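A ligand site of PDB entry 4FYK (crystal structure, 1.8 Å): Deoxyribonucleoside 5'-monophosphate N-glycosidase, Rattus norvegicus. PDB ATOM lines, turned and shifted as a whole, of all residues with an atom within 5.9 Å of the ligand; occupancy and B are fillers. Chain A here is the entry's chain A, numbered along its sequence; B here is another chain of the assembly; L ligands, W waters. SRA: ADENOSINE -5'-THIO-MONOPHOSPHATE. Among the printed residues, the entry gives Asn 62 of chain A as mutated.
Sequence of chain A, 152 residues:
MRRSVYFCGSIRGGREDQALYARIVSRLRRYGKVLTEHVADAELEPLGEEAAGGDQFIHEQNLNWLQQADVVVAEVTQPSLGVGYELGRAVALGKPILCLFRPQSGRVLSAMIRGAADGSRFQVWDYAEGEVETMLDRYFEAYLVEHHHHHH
OH of Tyr 6 touches O2' of the ligand, 3.7 Å away.
CA of Cys 8 touches O3' of the ligand, 3.4 Å away.
Ser 10 touches the ligand (CA to OP1, 3.9 Å).
Glu 37 touches the ligand.
CD2 of His 38 touches O3' of the ligand (3.7 Å).
Ile 58 touches the ligand.
Val 83 touches the ligand.
Met 112 of chain B touches the ligand.
18 residues have an atom within 4 Å of the ligand: Tyr 6, Cys 8, Gly 9, Ser 10, Ile 11, Arg 12, Gly 13, Glu 37, His 38, Ile 58, Asn 62, Ser 80, Gly 82, Val 83, Glu 86, Ser 110 of chain B, Ala 111 of chain B and Met 112 of chain B.
An oxygen (OP1) of the ligand lies within hydrogen-bond range of the backbone NH of Arg 12, 3.2 Å away.
The backbone carbonyl oxygen of Gly 9 is in hydrogen-bond range of an oxygen (O3') of the ligand, 3.2 Å away.
OE1 of Glu 86 is in hydrogen-bond range of O2' of the ligand (2.5 Å).
N of Ala 111 of chain B lies close to S2P of the ligand (3.5 Å).
An oxygen (OP3) of the ligand sits at hydrogen-bond distance from the side-chain hydroxyl (OG) of Ser 110 of chain B (2.7 Å).
The backbone NH (N) of Ile 11 lies within hydrogen-bond range of an oxygen (OP1) of the ligand, 2.9 Å away.
ND2 of Asn 62 is in hydrogen-bond range of N3 of the ligand (3.1 Å).
An oxygen (O3') of the ligand is in hydrogen-bond range of the backbone NH (N) of Gly 9 (3.0 Å).
The side-chain hydroxyl (OG) of Ser 80 is in hydrogen-bond range of an oxygen (OP1) of the ligand, 3.0 Å away.
The backbone NH of Gly 13 sits at hydrogen-bond distance from an oxygen (OP1) of the ligand.
N of Gly 82 sits at hydrogen-bond distance from OP3 of the ligand.
Water W1 bridges O2' of the ligand and O of Phe 7.
Water W4 lies within hydrogen-bond range of N7 of the ligand (2.8 Å) and NH2 of Arg 12 (3.2 Å).
Water W3 lies within hydrogen-bond range of N of Leu 81 (2.9 Å) and OP3 of the ligand (2.9 Å).
Water W5 lies within hydrogen-bond range of the side-chain amide oxygen (OD1) of Asn 62 (3.0 Å) and the backbone NH (N) of Glu 37 (3.1 Å).
N of Val 83 is in hydrogen-bond range of OG of Ser 80 (3.2 Å).
O of Gly 9 lies within hydrogen-bond range of NE2 of His 38, 2.6 Å away.
The side-chain carboxylate of Glu 86 sits at hydrogen-bond distance from the side-chain hydroxyl of Tyr 6 (2.6 Å).
OG of Ser 10 sits at hydrogen-bond distance from O of Gly 14 (2.8 Å).
OE2 of Glu 86 sits close to SG of Cys 8 (3.6 Å).
The side-chain hydroxyl (OG) of Ser 80 lies close to the backbone NH (N) of Gly 82 (3.3 Å).
The side-chain amide nitrogen (ND2) of Asn 62 sits at hydrogen-bond distance from the side-chain sulfur (SD) of Met 112 of chain B (3.6 Å).
The backbone NH (N) of Met 112 of chain B lies close to the side-chain hydroxyl (OG) of Ser 110 of chain B (3.3 Å).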
ATOM      1  N   TYR A   6       0.773 -15.213  -6.234  1.00  0.00           N
ATOM      2  CA  TYR A   6       2.195 -14.860  -6.311  1.00  0.00           C
ATOM      3  C   TYR A   6       3.027 -16.131  -6.115  1.00  0.00           C
ATOM      4  O   TYR A   6       2.878 -16.823  -5.083  1.00  0.00           O
ATOM      5  CB  TYR A   6       2.521 -13.858  -5.212  1.00  0.00           C
ATOM      6  CG  TYR A   6       3.926 -13.259  -5.259  1.00  0.00           C
ATOM      7  CD1 TYR A   6       4.127 -11.940  -5.686  1.00  0.00           C
ATOM      8  CD2 TYR A   6       5.025 -13.987  -4.818  1.00  0.00           C
ATOM      9  CE1 TYR A   6       5.390 -11.387  -5.708  1.00  0.00           C
ATOM     10  CE2 TYR A   6       6.302 -13.437  -4.838  1.00  0.00           C
ATOM     11  CZ  TYR A   6       6.475 -12.137  -5.287  1.00  0.00           C
ATOM     12  OH  TYR A   6       7.739 -11.584  -5.309  1.00  0.00           O
ATOM     13  N   PHE A   7       3.890 -16.444  -7.076  1.00  0.00           N
ATOM     14  CA  PHE A   7       4.758 -17.622  -6.966  1.00  0.00           C
ATOM     15  C   PHE A   7       6.205 -17.279  -6.602  1.00  0.00           C
ATOM     16  O   PHE A   7       6.786 -16.343  -7.165  1.00  0.00           O
ATOM     17  CB  PHE A   7       4.730 -18.463  -8.244  1.00  0.00           C
ATOM     18  CG  PHE A   7       5.728 -19.579  -8.212  1.00  0.00           C
ATOM     19  CD1 PHE A   7       6.981 -19.431  -8.781  1.00  0.00           C
ATOM     20  CD2 PHE A   7       5.438 -20.756  -7.527  1.00  0.00           C
ATOM     21  CE1 PHE A   7       7.931 -20.450  -8.714  1.00  0.00           C
ATOM     22  CE2 PHE A   7       6.377 -21.794  -7.456  1.00  0.00           C
ATOM     23  CZ  PHE A   7       7.628 -21.632  -8.043  1.00  0.00           C
ATOM     24  N   CYS A   8       6.781 -18.053  -5.670  1.00  0.00           N
ATOM     25  CA  CYS A   8       8.158 -17.861  -5.191  1.00  0.00           C
ATOM     26  C   CYS A   8       8.979 -19.111  -5.470  1.00  0.00           C
ATOM     27  O   CYS A   8       8.519 -20.225  -5.225  1.00  0.00           O
ATOM     28  CB  CYS A   8       8.235 -17.613  -3.661  1.00  0.00           C
ATOM     29  SG  CYS A   8       7.009 -16.547  -2.905  1.00  0.00           S
ATOM     30  N   GLY A   9      10.191 -18.938  -5.981  1.00  0.00           N
ATOM     31  CA  GLY A   9      11.083 -20.075  -6.229  1.00  0.00           C
ATOM     32  C   GLY A   9      12.494 -19.563  -6.405  1.00  0.00           C
ATOM     33  O   GLY A   9      12.687 -18.488  -6.984  1.00  0.00           O
ATOM     34  N   SER A  10      13.471 -20.320  -5.907  1.00  0.00           N
ATOM     35  CA  SER A  10      14.887 -19.945  -5.974  1.00  0.00           C
ATOM     36  C   SER A  10      15.350 -19.565  -7.396  1.00  0.00           C
ATOM     37  O   SER A  10      15.000 -20.216  -8.398  1.00  0.00           O
ATOM     38  CB  SER A  10      15.756 -21.076  -5.436  1.00  0.00           C
ATOM     39  OG  SER A  10      17.143 -20.757  -5.468  1.00  0.00           O
ATOM     40  N   ILE A  11      16.146 -18.497  -7.468  1.00  0.00           N
ATOM     41  CA  ILE A  11      16.788 -18.094  -8.711  1.00  0.00           C
ATOM     42  C   ILE A  11      18.308 -18.024  -8.493  1.00  0.00           C
ATOM     43  O   ILE A  11      19.030 -18.952  -8.880  1.00  0.00           O
ATOM     44  CB  ILE A  11      16.208 -16.761  -9.275  1.00  0.00           C
ATOM     45  CG1 ILE A  11      14.741 -16.976  -9.658  1.00  0.00           C
ATOM     46  CG2 ILE A  11      16.994 -16.318 -10.513  1.00  0.00           C
ATOM     47  CD1 ILE A  11      13.982 -15.722 -10.076  1.00  0.00           C
ATOM     48  N   ARG A  12      18.802 -16.961  -7.869  1.00  0.00           N
ATOM     49  CA  ARG A  12      20.242 -16.874  -7.582  1.00  0.00           C
ATOM     50  C   ARG A  12      20.646 -17.820  -6.458  1.00  0.00           C
ATOM     51  O   ARG A  12      21.816 -18.161  -6.314  1.00  0.00           O
ATOM     52  CB  ARG A  12      20.658 -15.443  -7.249  1.00  0.00           C
ATOM     53  CG  ARG A  12      20.408 -14.500  -8.390  1.00  0.00           C
ATOM     54  CD  ARG A  12      20.867 -13.085  -8.121  1.00  0.00           C
ATOM     55  NE  ARG A  12      20.376 -12.200  -9.166  1.00  0.00           N
ATOM     56  CZ  ARG A  12      20.329 -10.858  -9.076  1.00  0.00           C
ATOM     57  NH1 ARG A  12      20.775 -10.220  -8.001  1.00  0.00           N
ATOM     58  NH2 ARG A  12      19.830 -10.164 -10.079  1.00  0.00           N
ATOM     59  N   GLY A  13      19.667 -18.248  -5.647  1.00  0.00           N
ATOM     60  CA  GLY A  13      19.894 -19.321  -4.676  1.00  0.00           C
ATOM     61  C   GLY A  13      20.291 -20.634  -5.331  1.00  0.00           C
ATOM     62  O   GLY A  13      20.848 -21.524  -4.679  1.00  0.00           O
ATOM     63  N   GLY A  14      19.978 -20.774  -6.621  1.00  0.00           N
ATOM     64  CA  GLY A  14      20.236 -22.000  -7.365  1.00  0.00           C
ATOM     65  C   GLY A  14      19.025 -22.316  -8.213  1.00  0.00           C
ATOM     66  O   GLY A  14      17.888 -22.196  -7.748  1.00  0.00           O
ATOM     67  N   THR A  36       3.230 -12.959 -10.939  1.00  0.00           N
ATOM     68  CA  THR A  36       4.671 -12.961 -10.992  1.00  0.00           C
ATOM     69  C   THR A  36       5.185 -13.242 -12.397  1.00  0.00           C
ATOM     70  O   THR A  36       4.541 -13.945 -13.182  1.00  0.00           O
ATOM     71  CB  THR A  36       5.280 -13.929  -9.954  1.00  0.00           C
ATOM     72  OG1 THR A  36       4.474 -15.114  -9.839  1.00  0.00           O
ATOM     73  CG2 THR A  36       5.341 -13.246  -8.587  1.00  0.00           C
ATOM     74  N   GLU A  37       6.338 -12.644 -12.692  1.00  0.00           N
ATOM     75  CA  GLU A  37       7.083 -12.927 -13.898  1.00  0.00           C
ATOM     76  C   GLU A  37       8.434 -13.506 -13.485  1.00  0.00           C
ATOM     77  O   GLU A  37       9.508 -12.986 -13.818  1.00  0.00           O
ATOM     78  CB  GLU A  37       7.233 -11.660 -14.760  1.00  0.00           C
ATOM     79  CG  GLU A  37       5.889 -11.173 -15.273  1.00  0.00           C
ATOM     80  CD  GLU A  37       5.972  -9.883 -16.052  1.00  0.00           C
ATOM     81  OE1 GLU A  37       7.100  -9.383 -16.283  1.00  0.00           O
ATOM     82  OE2 GLU A  37       4.905  -9.360 -16.439  1.00  0.00           O
ATOM     83  N   HIS A  38       8.342 -14.596 -12.721  1.00  0.00           N
ATOM     84  CA  HIS A  38       9.491 -15.373 -12.280  1.00  0.00           C
ATOM     85  C   HIS A  38      10.338 -15.822 -13.473  1.00  0.00           C
ATOM     86  O   HIS A  38      11.565 -15.661 -13.474  1.00  0.00           O
ATOM     87  CB  HIS A  38       8.992 -16.596 -11.505  1.00  0.00           C
ATOM     88  CG  HIS A  38      10.057 -17.317 -10.731  1.00  0.00           C
ATOM     89  ND1 HIS A  38      10.924 -18.204 -11.316  1.00  0.00           N
ATOM     90  CD2 HIS A  38      10.371 -17.281  -9.414  1.00  0.00           C
ATOM     91  CE1 HIS A  38      11.744 -18.679 -10.393  1.00  0.00           C
ATOM     92  NE2 HIS A  38      11.429 -18.141  -9.227  1.00  0.00           N
ATOM     93  N   ILE A  58      13.436  -4.883  -9.548  1.00  0.00           N
ATOM     94  CA  ILE A  58      12.881  -6.216  -9.281  1.00  0.00           C
ATOM     95  C   ILE A  58      12.180  -6.205  -7.934  1.00  0.00           C
ATOM     96  O   ILE A  58      11.048  -6.658  -7.820  1.00  0.00           O
ATOM     97  CB  ILE A  58      13.967  -7.316  -9.341  1.00  0.00           C
ATOM     98  CG1 ILE A  58      14.514  -7.457 -10.761  1.00  0.00           C
ATOM     99  CG2 ILE A  58      13.419  -8.668  -8.857  1.00  0.00           C
ATOM    100  CD1 ILE A  58      15.733  -8.363 -10.826  1.00  0.00           C
ATOM    101  N   GLN A  61       8.877  -3.906  -7.999  1.00  0.00           N
ATOM    102  CA  GLN A  61       7.886  -4.600  -8.831  1.00  0.00           C
ATOM    103  C   GLN A  61       7.267  -5.786  -8.086  1.00  0.00           C
ATOM    104  O   GLN A  61       6.040  -6.000  -8.092  1.00  0.00           O
ATOM    105  CB  GLN A  61       8.572  -5.098 -10.109  1.00  0.00           C
ATOM    106  CG  GLN A  61       7.726  -6.026 -11.000  1.00  0.00           C
ATOM    107  CD  GLN A  61       8.545  -6.702 -12.103  1.00  0.00           C
ATOM    108  OE1 GLN A  61       8.383  -6.378 -13.278  1.00  0.00           O
ATOM    109  NE2 GLN A  61       9.411  -7.644 -11.726  1.00  0.00           N
ATOM    110  N   ASN A  62       8.123  -6.569  -7.433  1.00  0.00           N
ATOM    111  CA  ASN A  62       7.677  -7.752  -6.725  1.00  0.00           C
ATOM    112  C   ASN A  62       6.870  -7.415  -5.481  1.00  0.00           C
ATOM    113  O   ASN A  62       5.859  -8.058  -5.217  1.00  0.00           O
ATOM    114  CB  ASN A  62       8.830  -8.698  -6.391  1.00  0.00           C
ATOM    115  CG  ASN A  62       9.249  -9.561  -7.583  1.00  0.00           C
ATOM    116  OD1 ASN A  62       8.644  -9.501  -8.645  1.00  0.00           O
ATOM    117  ND2 ASN A  62      10.274 -10.365  -7.401  1.00  0.00           N
ATOM    118  N   TRP A  65       3.450  -6.532  -6.504  1.00  0.00           N
ATOM    119  CA  TRP A  65       2.703  -7.748  -6.807  1.00  0.00           C
ATOM    120  C   TRP A  65       2.290  -8.494  -5.530  1.00  0.00           C
ATOM    121  O   TRP A  65       1.163  -8.984  -5.433  1.00  0.00           O
ATOM    122  CB  TRP A  65       3.520  -8.667  -7.723  1.00  0.00           C
ATOM    123  CG  TRP A  65       3.501  -8.230  -9.154  1.00  0.00           C
ATOM    124  CD1 TRP A  65       2.532  -7.497  -9.779  1.00  0.00           C
ATOM    125  CD2 TRP A  65       4.476  -8.516 -10.161  1.00  0.00           C
ATOM    126  NE1 TRP A  65       2.839  -7.309 -11.089  1.00  0.00           N
ATOM    127  CE2 TRP A  65       4.034  -7.929 -11.362  1.00  0.00           C
ATOM    128  CE3 TRP A  65       5.691  -9.209 -10.163  1.00  0.00           C
ATOM    129  CZ2 TRP A  65       4.750  -8.011 -12.550  1.00  0.00           C
ATOM    130  CZ3 TRP A  65       6.406  -9.307 -11.358  1.00  0.00           C
ATOM    131  CH2 TRP A  65       5.925  -8.703 -12.530  1.00  0.00           C
ATOM    132  N   SER A  80      16.979 -20.366  -0.413  1.00  0.00           N
ATOM    133  CA  SER A  80      17.051 -19.109  -1.154  1.00  0.00           C
ATOM    134  C   SER A  80      16.645 -17.941  -0.258  1.00  0.00           C
ATOM    135  O   SER A  80      15.577 -17.971   0.360  1.00  0.00           O
ATOM    136  CB  SER A  80      16.127 -19.155  -2.372  1.00  0.00           C
ATOM    137  OG  SER A  80      15.751 -17.850  -2.731  1.00  0.00           O
ATOM    138  N   LEU A  81      17.504 -16.926  -0.181  1.00  0.00           N
ATOM    139  CA  LEU A  81      17.233 -15.755   0.642  1.00  0.00           C
ATOM    140  C   LEU A  81      15.980 -15.020   0.172  1.00  0.00           C
ATOM    141  O   LEU A  81      15.163 -14.559   0.985  1.00  0.00           O
ATOM    142  CB  LEU A  81      18.409 -14.781   0.633  1.00  0.00           C
ATOM    143  CG  LEU A  81      19.722 -15.223   1.259  1.00  0.00           C
ATOM    144  CD1 LEU A  81      20.861 -14.327   0.739  1.00  0.00           C
ATOM    145  CD2 LEU A  81      19.640 -15.157   2.784  1.00  0.00           C
ATOM    146  N   GLY A  82      15.816 -14.937  -1.148  1.00  0.00           N
ATOM    147  CA  GLY A  82      14.749 -14.141  -1.735  1.00  0.00           C
ATOM    148  C   GLY A  82      13.385 -14.770  -1.513  1.00  0.00           C
ATOM    149  O   GLY A  82      12.404 -14.069  -1.276  1.00  0.00           O
ATOM    150  N   VAL A  83      13.322 -16.103  -1.632  1.00  0.00           N
ATOM    151  CA  VAL A  83      12.103 -16.854  -1.297  1.00  0.00           C
ATOM    152  C   VAL A  83      11.732 -16.651   0.175  1.00  0.00           C
ATOM    153  O   VAL A  83      10.595 -16.310   0.491  1.00  0.00           O
ATOM    154  CB  VAL A  83      12.228 -18.358  -1.642  1.00  0.00           C
ATOM    155  CG1 VAL A  83      10.981 -19.115  -1.177  1.00  0.00           C
ATOM    156  CG2 VAL A  83      12.459 -18.563  -3.153  1.00  0.00           C
ATOM    157  N   GLU A  86      10.466 -13.005   0.597  1.00  0.00           N
ATOM    158  CA  GLU A  86       9.101 -12.875   0.092  1.00  0.00           C
ATOM    159  C   GLU A  86       8.078 -13.457   1.079  1.00  0.00           C
ATOM    160  O   GLU A  86       7.015 -12.847   1.331  1.00  0.00           O
ATOM    161  CB  GLU A  86       8.985 -13.579  -1.273  1.00  0.00           C
ATOM    162  CG  GLU A  86       9.678 -12.825  -2.389  1.00  0.00           C
ATOM    163  CD  GLU A  86       9.861 -13.639  -3.692  1.00  0.00           C
ATOM    164  OE1 GLU A  86       9.832 -12.980  -4.770  1.00  0.00           O
ATOM    165  OE2 GLU A  86      10.084 -14.894  -3.654  1.00  0.00           O
ATOM    166  N   LEU B 109      24.523 -12.156  -5.132  1.00  0.00           N
ATOM    167  CA  LEU B 109      23.570 -12.017  -4.043  1.00  0.00           C
ATOM    168  C   LEU B 109      22.156 -11.861  -4.585  1.00  0.00           C
ATOM    169  O   LEU B 109      21.943 -11.125  -5.561  1.00  0.00           O
ATOM    170  CB  LEU B 109      23.909 -10.836  -3.132  1.00  0.00           C
ATOM    171  CG  LEU B 109      22.913 -10.552  -1.988  1.00  0.00           C
ATOM    172  CD1 LEU B 109      22.847 -11.744  -0.976  1.00  0.00           C
ATOM    173  CD2 LEU B 109      23.250  -9.250  -1.267  1.00  0.00           C
ATOM    174  N   SER B 110      21.229 -12.587  -3.948  1.00  0.00           N
ATOM    175  CA  SER B 110      19.781 -12.467  -4.110  1.00  0.00           C
ATOM    176  C   SER B 110      19.318 -11.095  -4.586  1.00  0.00           C
ATOM    177  O   SER B 110      19.660 -10.083  -3.969  1.00  0.00           O
ATOM    178  CB  SER B 110      19.100 -12.745  -2.766  1.00  0.00           C
ATOM    179  OG  SER B 110      17.703 -12.488  -2.830  1.00  0.00           O
ATOM    180  N   ALA B 111      18.519 -11.071  -5.649  1.00  0.00           N
ATOM    181  CA  ALA B 111      17.956  -9.830  -6.178  1.00  0.00           C
ATOM    182  C   ALA B 111      17.051  -9.146  -5.170  1.00  0.00           C
ATOM    183  O   ALA B 111      16.955  -7.916  -5.160  1.00  0.00           O
ATOM    184  CB  ALA B 111      17.164 -10.116  -7.468  1.00  0.00           C
ATOM    185  N   MET B 112      16.382  -9.916  -4.330  1.00  0.00           N
ATOM    186  CA  MET B 112      15.485  -9.351  -3.353  1.00  0.00           C
ATOM    187  C   MET B 112      16.239  -8.706  -2.201  1.00  0.00           C
ATOM    188  O   MET B 112      15.796  -7.703  -1.664  1.00  0.00           O
ATOM    189  CB  MET B 112      14.507 -10.395  -2.812  1.00  0.00           C
ATOM    190  CG  MET B 112      13.542 -10.913  -3.871  1.00  0.00           C
ATOM    191  SD  MET B 112      12.550  -9.644  -4.693  1.00  0.00           S
ATOM    192  CE  MET B 112      11.391  -9.197  -3.401  1.00  0.00           C
HETATM  193  P   SRA L   1      16.712 -15.456  -4.859  1.00  0.00           P
HETATM  194  OP1 SRA L   1      17.009 -16.798  -5.262  1.00  0.00           O
HETATM  195  S2P SRA L   1      17.317 -14.299  -6.402  1.00  0.00           S
HETATM  196  OP3 SRA L   1      17.468 -15.017  -3.741  1.00  0.00           O
HETATM  197  O5' SRA L   1      15.276 -15.177  -4.736  1.00  0.00           O
HETATM  198  C5' SRA L   1      14.306 -15.692  -5.661  1.00  0.00           C
HETATM  199  C4' SRA L   1      13.055 -14.832  -5.679  1.00  0.00           C
HETATM  200  O4' SRA L   1      13.436 -13.519  -6.102  1.00  0.00           O
HETATM  201  C3' SRA L   1      12.016 -15.375  -6.656  1.00  0.00           C
HETATM  202  O3' SRA L   1      10.950 -16.075  -5.940  1.00  0.00           O
HETATM  203  C2' SRA L   1      11.538 -14.172  -7.453  1.00  0.00           C
HETATM  204  C1' SRA L   1      12.561 -13.063  -7.168  1.00  0.00           C
HETATM  205  N9  SRA L   1      13.411 -12.736  -8.333  1.00  0.00           N
HETATM  206  C8  SRA L   1      14.730 -12.842  -8.500  1.00  0.00           C
HETATM  207  N7  SRA L   1      15.056 -12.401  -9.715  1.00  0.00           N
HETATM  208  C5  SRA L   1      13.917 -12.020 -10.309  1.00  0.00           C
HETATM  209  C6  SRA L   1      13.659 -11.514 -11.524  1.00  0.00           C
HETATM  210  N6  SRA L   1      14.665 -11.304 -12.359  1.00  0.00           N
HETATM  211  N1  SRA L   1      12.436 -11.188 -11.899  1.00  0.00           N
HETATM  212  C2  SRA L   1      11.261 -11.386 -11.038  1.00  0.00           C
HETATM  213  N3  SRA L   1      11.636 -11.934  -9.729  1.00  0.00           N
HETATM  214  C4  SRA L   1      12.915 -12.227  -9.451  1.00  0.00           C
HETATM  215  O2' SRA L   1      10.197 -13.740  -7.078  1.00  0.00           O
HETATM  216  O   HOH W   1       8.510 -14.617  -8.670  1.00  0.00           O
HETATM  217  O   HOH W   2      14.640  -9.882 -15.109  1.00  0.00           O
HETATM  218  O   HOH W   3      19.364 -16.652  -2.337  1.00  0.00           O
HETATM  219  O   HOH W   4      17.514 -12.102 -11.112  1.00  0.00           O
HETATM  220  O   HOH W   5       8.076 -12.016 -10.209  1.00  0.00           O
